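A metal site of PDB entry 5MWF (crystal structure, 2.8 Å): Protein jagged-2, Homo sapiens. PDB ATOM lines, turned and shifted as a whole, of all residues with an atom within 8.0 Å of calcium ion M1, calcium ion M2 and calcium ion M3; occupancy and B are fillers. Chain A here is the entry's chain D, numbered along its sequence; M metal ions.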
ATOM      1  N   LEU A  18       6.179  15.115 -29.290  1.00  0.00           N
ATOM      2  CA  LEU A  18       6.893  14.402 -30.345  1.00  0.00           C
ATOM      3  C   LEU A  18       5.881  13.680 -31.228  1.00  0.00           C
ATOM      4  O   LEU A  18       4.674  13.697 -30.975  1.00  0.00           O
ATOM      5  CB  LEU A  18       7.906  13.416 -29.771  1.00  0.00           C
ATOM      6  CG  LEU A  18       8.720  13.827 -28.543  1.00  0.00           C
ATOM      7  CD1 LEU A  18       9.284  12.608 -27.848  1.00  0.00           C
ATOM      8  CD2 LEU A  18       9.842  14.750 -28.947  1.00  0.00           C
ATOM      9  N   CYS A  23       5.019  13.887 -24.373  1.00  0.00           N
ATOM     10  CA  CYS A  23       5.649  15.190 -24.275  1.00  0.00           C
ATOM     11  C   CYS A  23       7.162  15.057 -24.376  1.00  0.00           C
ATOM     12  O   CYS A  23       7.735  13.975 -24.215  1.00  0.00           O
ATOM     13  CB  CYS A  23       5.234  15.893 -22.972  1.00  0.00           C
ATOM     14  SG  CYS A  23       3.619  16.726 -23.103  1.00  0.00           S
ATOM     15  N   CYS A  24       7.821  16.182 -24.673  1.00  0.00           N
ATOM     16  CA  CYS A  24       9.242  16.207 -25.012  1.00  0.00           C
ATOM     17  C   CYS A  24      10.127  15.838 -23.835  1.00  0.00           C
ATOM     18  O   CYS A  24      10.138  14.693 -23.385  1.00  0.00           O
ATOM     19  CB  CYS A  24       9.632  17.593 -25.513  1.00  0.00           C
ATOM     20  SG  CYS A  24      10.057  17.686 -27.254  1.00  0.00           S
ATOM     21  N   ASP A  25      10.899  16.809 -23.359  1.00  0.00           N
ATOM     22  CA  ASP A  25      11.787  16.588 -22.222  1.00  0.00           C
ATOM     23  C   ASP A  25      10.993  16.248 -20.963  1.00  0.00           C
ATOM     24  O   ASP A  25       9.772  16.433 -20.929  1.00  0.00           O
ATOM     25  CB  ASP A  25      12.653  17.834 -21.978  1.00  0.00           C
ATOM     26  CG  ASP A  25      13.934  17.831 -22.800  1.00  0.00           C
ATOM     27  OD1 ASP A  25      14.284  16.775 -23.353  1.00  0.00           O
ATOM     28  OD2 ASP A  25      14.583  18.898 -22.881  1.00  0.00           O
ATOM     29  N   HIS A  38       7.474  22.604 -18.738  1.00  0.00           N
ATOM     30  CA  HIS A  38       8.096  23.906 -18.896  1.00  0.00           C
ATOM     31  C   HIS A  38       9.517  23.847 -19.453  1.00  0.00           C
ATOM     32  O   HIS A  38       9.920  24.791 -20.154  1.00  0.00           O
ATOM     33  CB  HIS A  38       8.113  24.675 -17.572  1.00  0.00           C
ATOM     34  CG  HIS A  38       6.952  25.610 -17.387  1.00  0.00           C
ATOM     35  ND1 HIS A  38       6.850  26.805 -18.070  1.00  0.00           N
ATOM     36  CD2 HIS A  38       5.848  25.514 -16.608  1.00  0.00           C
ATOM     37  CE1 HIS A  38       5.727  27.413 -17.708  1.00  0.00           C
ATOM     38  NE2 HIS A  38       5.109  26.655 -16.834  1.00  0.00           N
ATOM     39  N   ASP A  39      10.282  22.796 -19.171  1.00  0.00           N
ATOM     40  CA  ASP A  39      11.567  22.604 -19.862  1.00  0.00           C
ATOM     41  C   ASP A  39      11.255  22.066 -21.249  1.00  0.00           C
ATOM     42  O   ASP A  39      10.953  20.881 -21.426  1.00  0.00           O
ATOM     43  CB  ASP A  39      12.495  21.657 -19.116  1.00  0.00           C
ATOM     44  CG  ASP A  39      13.855  21.534 -19.816  1.00  0.00           C
ATOM     45  OD1 ASP A  39      14.709  20.708 -19.413  1.00  0.00           O
ATOM     46  OD2 ASP A  39      14.087  22.289 -20.779  1.00  0.00           O
ATOM     47  N   GLU A  40      11.370  22.942 -22.245  1.00  0.00           N
ATOM     48  CA  GLU A  40      10.900  22.653 -23.595  1.00  0.00           C
ATOM     49  C   GLU A  40      11.836  21.669 -24.287  1.00  0.00           C
ATOM     50  O   GLU A  40      12.880  21.256 -23.758  1.00  0.00           O
ATOM     51  CB  GLU A  40      10.801  23.941 -24.399  1.00  0.00           C
ATOM     52  CG  GLU A  40       9.820  24.963 -23.824  1.00  0.00           C
ATOM     53  CD  GLU A  40      10.143  26.376 -24.291  1.00  0.00           C
ATOM     54  OE1 GLU A  40      11.318  26.641 -24.621  1.00  0.00           O
ATOM     55  OE2 GLU A  40       9.214  27.206 -24.339  1.00  0.00           O
ATOM     56  N   CYS A  41      11.445  21.292 -25.509  1.00  0.00           N
ATOM     57  CA  CYS A  41      12.344  20.573 -26.397  1.00  0.00           C
ATOM     58  C   CYS A  41      13.561  21.432 -26.685  1.00  0.00           C
ATOM     59  O   CYS A  41      13.463  22.660 -26.786  1.00  0.00           O
ATOM     60  CB  CYS A  41      11.643  20.224 -27.714  1.00  0.00           C
ATOM     61  SG  CYS A  41       9.933  19.670 -27.637  1.00  0.00           S
ATOM     62  N   ASP A  42      14.703  20.778 -26.835  1.00  0.00           N
ATOM     63  CA  ASP A  42      15.932  21.434 -27.254  1.00  0.00           C
ATOM     64  C   ASP A  42      16.256  20.864 -28.640  1.00  0.00           C
ATOM     65  O   ASP A  42      16.970  19.867 -28.766  1.00  0.00           O
ATOM     66  CB  ASP A  42      17.042  21.210 -26.223  1.00  0.00           C
ATOM     67  CG  ASP A  42      16.518  21.264 -24.779  1.00  0.00           C
ATOM     68  OD1 ASP A  42      16.178  22.353 -24.287  1.00  0.00           O
ATOM     69  OD2 ASP A  42      16.424  20.205 -24.125  1.00  0.00           O
ATOM     70  N   THR A  43      15.707  21.505 -29.666  1.00  0.00           N
ATOM     71  CA  THR A  43      15.577  20.890 -30.986  1.00  0.00           C
ATOM     72  C   THR A  43      16.725  21.239 -31.920  1.00  0.00           C
ATOM     73  O   THR A  43      17.196  22.380 -31.959  1.00  0.00           O
ATOM     74  CB  THR A  43      14.258  21.307 -31.653  1.00  0.00           C
ATOM     75  OG1 THR A  43      14.445  22.572 -32.294  1.00  0.00           O
ATOM     76  CG2 THR A  43      13.157  21.434 -30.622  1.00  0.00           C
ATOM     77  N   TYR A  44      17.170  20.230 -32.670  1.00  0.00           N
ATOM     78  CA  TYR A  44      18.088  20.366 -33.789  1.00  0.00           C
ATOM     79  C   TYR A  44      17.487  19.619 -34.974  1.00  0.00           C
ATOM     80  O   TYR A  44      16.495  18.905 -34.832  1.00  0.00           O
ATOM     81  CB  TYR A  44      19.480  19.825 -33.446  1.00  0.00           C
ATOM     82  CG  TYR A  44      19.493  18.336 -33.185  1.00  0.00           C
ATOM     83  CD1 TYR A  44      19.090  17.813 -31.959  1.00  0.00           C
ATOM     84  CD2 TYR A  44      19.900  17.444 -34.168  1.00  0.00           C
ATOM     85  CE1 TYR A  44      19.090  16.449 -31.726  1.00  0.00           C
ATOM     86  CE2 TYR A  44      19.900  16.085 -33.943  1.00  0.00           C
ATOM     87  CZ  TYR A  44      19.500  15.587 -32.717  1.00  0.00           C
ATOM     88  OH  TYR A  44      19.510  14.234 -32.501  1.00  0.00           O
ATOM     89  N   VAL A  71      21.646  22.635 -31.453  1.00  0.00           N
ATOM     90  CA  VAL A  71      20.331  22.992 -30.939  1.00  0.00           C
ATOM     91  C   VAL A  71      20.053  24.461 -31.229  1.00  0.00           C
ATOM     92  O   VAL A  71      20.859  25.341 -30.907  1.00  0.00           O
ATOM     93  CB  VAL A  71      20.243  22.695 -29.431  1.00  0.00           C
ATOM     94  CG1 VAL A  71      18.922  23.211 -28.863  1.00  0.00           C
ATOM     95  CG2 VAL A  71      20.377  21.199 -29.180  1.00  0.00           C
ATOM     96  N   GLY A  73      16.908  26.164 -30.594  1.00  0.00           N
ATOM     97  CA  GLY A  73      15.984  26.871 -29.725  1.00  0.00           C
ATOM     98  C   GLY A  73      15.108  25.908 -28.956  1.00  0.00           C
ATOM     99  O   GLY A  73      15.450  24.738 -28.776  1.00  0.00           O
ATOM    100  N   GLY A  74      13.958  26.419 -28.509  1.00  0.00           N
ATOM    101  CA  GLY A  74      13.030  25.622 -27.739  1.00  0.00           C
ATOM    102  C   GLY A  74      11.975  24.955 -28.597  1.00  0.00           C
ATOM    103  O   GLY A  74      12.283  24.377 -29.632  1.00  0.00           O
ATOM    104  N   ASN A  75      10.706  25.036 -28.159  1.00  0.00           N
ATOM    105  CA  ASN A  75       9.617  24.478 -28.955  1.00  0.00           C
ATOM    106  C   ASN A  75       9.451  25.237 -30.259  1.00  0.00           C
ATOM    107  O   ASN A  75       9.393  24.631 -31.339  1.00  0.00           O
ATOM    108  CB  ASN A  75       8.311  24.501 -28.146  1.00  0.00           C
ATOM    109  CG  ASN A  75       8.301  23.489 -27.023  1.00  0.00           C
ATOM    110  OD1 ASN A  75       9.031  22.496 -27.070  1.00  0.00           O
ATOM    111  ND2 ASN A  75       7.478  23.727 -26.021  1.00  0.00           N
ATOM    112  N   TRP A 123      14.645  16.763 -34.112  1.00  0.00           N
ATOM    113  CA  TRP A 123      14.919  15.840 -33.016  1.00  0.00           C
ATOM    114  C   TRP A 123      15.036  16.610 -31.712  1.00  0.00           C
ATOM    115  O   TRP A 123      15.194  17.832 -31.687  1.00  0.00           O
ATOM    116  CB  TRP A 123      16.217  15.042 -33.254  1.00  0.00           C
ATOM    117  CG  TRP A 123      16.145  14.069 -34.388  1.00  0.00           C
ATOM    118  CD1 TRP A 123      16.302  14.345 -35.717  1.00  0.00           C
ATOM    119  CD2 TRP A 123      15.900  12.657 -34.307  1.00  0.00           C
ATOM    120  NE1 TRP A 123      16.163  13.197 -36.460  1.00  0.00           N
ATOM    121  CE2 TRP A 123      15.917  12.143 -35.618  1.00  0.00           C
ATOM    122  CE3 TRP A 123      15.656  11.778 -33.237  1.00  0.00           C
ATOM    123  CZ2 TRP A 123      15.705  10.794 -35.894  1.00  0.00           C
ATOM    124  CZ3 TRP A 123      15.462  10.439 -33.519  1.00  0.00           C
ATOM    125  CH2 TRP A 123      15.480   9.962 -34.835  1.00  0.00           C
ATOM    126  N   ASP A 124      14.945  15.867 -30.606  1.00  0.00           N
ATOM    127  CA  ASP A 124      15.192  16.402 -29.266  1.00  0.00           C
ATOM    128  C   ASP A 124      16.561  15.935 -28.800  1.00  0.00           C
ATOM    129  O   ASP A 124      16.989  14.817 -29.081  1.00  0.00           O
ATOM    130  CB  ASP A 124      14.113  15.940 -28.285  1.00  0.00           C
ATOM    131  CG  ASP A 124      14.434  16.315 -26.843  1.00  0.00           C
ATOM    132  OD1 ASP A 124      14.915  17.435 -26.604  1.00  0.00           O
ATOM    133  OD2 ASP A 124      14.211  15.466 -25.947  1.00  0.00           O
ATOM    134  N   TRP A 125      17.257  16.802 -28.066  1.00  0.00           N
ATOM    135  CA  TRP A 125      18.605  16.534 -27.593  1.00  0.00           C
ATOM    136  C   TRP A 125      18.581  16.279 -26.096  1.00  0.00           C
ATOM    137  O   TRP A 125      18.128  17.133 -25.321  1.00  0.00           O
ATOM    138  CB  TRP A 125      19.546  17.696 -27.932  1.00  0.00           C
ATOM    139  CG  TRP A 125      20.996  17.397 -27.682  1.00  0.00           C
ATOM    140  CD1 TRP A 125      21.823  18.038 -26.809  1.00  0.00           C
ATOM    141  CD2 TRP A 125      21.792  16.387 -28.312  1.00  0.00           C
ATOM    142  NE1 TRP A 125      23.081  17.500 -26.857  1.00  0.00           N
ATOM    143  CE2 TRP A 125      23.091  16.482 -27.777  1.00  0.00           C
ATOM    144  CE3 TRP A 125      21.544  15.411 -29.286  1.00  0.00           C
ATOM    145  CZ2 TRP A 125      24.135  15.638 -28.177  1.00  0.00           C
ATOM    146  CZ3 TRP A 125      22.571  14.580 -29.680  1.00  0.00           C
ATOM    147  CH2 TRP A 125      23.851  14.694 -29.126  1.00  0.00           C
ATOM    148  N   ASP A 126      19.074  15.105 -25.681  1.00  0.00           N
ATOM    149  CA  ASP A 126      19.234  14.757 -24.280  1.00  0.00           C
ATOM    150  C   ASP A 126      20.700  14.515 -23.914  1.00  0.00           C
ATOM    151  O   ASP A 126      20.997  13.779 -22.972  1.00  0.00           O
ATOM    152  CB  ASP A 126      18.385  13.530 -23.926  1.00  0.00           C
ATOM    153  CG  ASP A 126      16.890  13.840 -23.938  1.00  0.00           C
ATOM    154  OD1 ASP A 126      16.533  15.014 -23.740  1.00  0.00           O
ATOM    155  OD2 ASP A 126      16.094  12.902 -24.154  1.00  0.00           O
ATOM    156  N   ASN A 127      21.613  15.115 -24.678  1.00  0.00           N
ATOM    157  CA  ASN A 127      23.047  15.159 -24.397  1.00  0.00           C
ATOM    158  C   ASN A 127      23.737  13.797 -24.466  1.00  0.00           C
ATOM    159  O   ASN A 127      24.971  13.726 -24.357  1.00  0.00           O
ATOM    160  CB  ASN A 127      23.295  15.804 -23.016  1.00  0.00           C
ATOM    161  CG  ASN A 127      23.012  17.299 -23.016  1.00  0.00           C
ATOM    162  OD1 ASN A 127      21.869  17.727 -22.885  1.00  0.00           O
ATOM    163  ND2 ASN A 127      24.064  18.100 -23.170  1.00  0.00           N
ATOM    164  N   GLU A 134      12.583   7.052 -30.660  1.00  0.00           N
ATOM    165  CA  GLU A 134      11.365   7.592 -30.056  1.00  0.00           C
ATOM    166  C   GLU A 134      11.505   9.035 -29.593  1.00  0.00           C
ATOM    167  O   GLU A 134      10.678   9.514 -28.808  1.00  0.00           O
ATOM    168  CB  GLU A 134      10.926   6.709 -28.893  1.00  0.00           C
ATOM    169  CG  GLU A 134      10.667   5.266 -29.282  1.00  0.00           C
ATOM    170  CD  GLU A 134       9.751   4.553 -28.306  1.00  0.00           C
ATOM    171  OE1 GLU A 134       8.630   4.153 -28.716  1.00  0.00           O
ATOM    172  OE2 GLU A 134      10.131   4.405 -27.124  1.00  0.00           O
ATOM    173  N   LEU A 135      12.527   9.746 -30.079  1.00  0.00           N
ATOM    174  CA  LEU A 135      12.716  11.164 -29.793  1.00  0.00           C
ATOM    175  C   LEU A 135      12.589  12.035 -31.031  1.00  0.00           C
ATOM    176  O   LEU A 135      12.936  13.218 -30.987  1.00  0.00           O
ATOM    177  CB  LEU A 135      14.068  11.397 -29.135  1.00  0.00           C
ATOM    178  CG  LEU A 135      14.507  10.358 -28.102  1.00  0.00           C
ATOM    179  CD1 LEU A 135      16.014  10.464 -27.867  1.00  0.00           C
ATOM    180  CD2 LEU A 135      13.739  10.519 -26.791  1.00  0.00           C
HETATM  181 CA    CA M   1      14.272  14.411 -23.822  1.00  0.00          CA
HETATM  182 CA    CA M   2      14.973  21.115 -22.184  1.00  0.00          CA
HETATM  183 CA    CA M   3      16.066  17.863 -24.481  1.00  0.00          CA
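The backbone NH (N) of Asp 124 lies within hydrogen-bond range of the backbone carbonyl oxygen (O) of Leu 135 (3.3 Å).
The side-chain sulfur of Cys 24 is disulfide-bonded to the side-chain sulfur of Cys 41 (2.0 Å).
Three residues have an atom within 4 Å of calcium ion M1: Asp 25, Asp 124 and Asp 126.
Along chain A the residues within 4 Å of calcium ion M1 span positions 25 to 126.
The nearest printed residue that does not touch calcium ion M1 is Cys 24 (4.2 Å).
The nearest printed residue that does not touch calcium ion M2 is Cys 41 (4.7 Å).
Five residues have an atom within 4 Å of calcium ion M3: Asp 25, Asp 42, Asp 124, Trp 125 and Asp 126.
Calcium ion M1 is bound by OD1 of Asp 126 (2.3 Å), OD2 of Asp 124 (2.4 Å), OD2 of Asp 126 (2.4 Å) and OD1 of Asp 25 (2.4 Å).
Calcium ion M2 is bound by the side-chain carboxylate (OD2) of Asp 39 (2.0 Å), the side-chain carboxylate (OD2) of Asp 25 (2.4 Å), the side-chain carboxylate (OD2) of Asp 42 (2.6 Å), the backbone carbonyl oxygen (O) of Glu 40 (2.6 Å), the side-chain carboxylate (OD1) of Asp 42 (2.7 Å) and the side-chain carboxylate (OD1) of Asp 39 (2.8 Å).
Calcium ion M2 has six donor atoms within binding distance.
Calcium ion M3 is bound by O of Trp 125 (2.3 Å), OD1 of Asp 25 (2.4 Å), OD2 of Asp 42 (2.4 Å), OD2 of Asp 25 (2.4 Å) and OD1 of Asp 124 (2.5 Å).
Slightly farther from calcium ion M3 lies OD1 of Asp 126 (3.0 Å).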
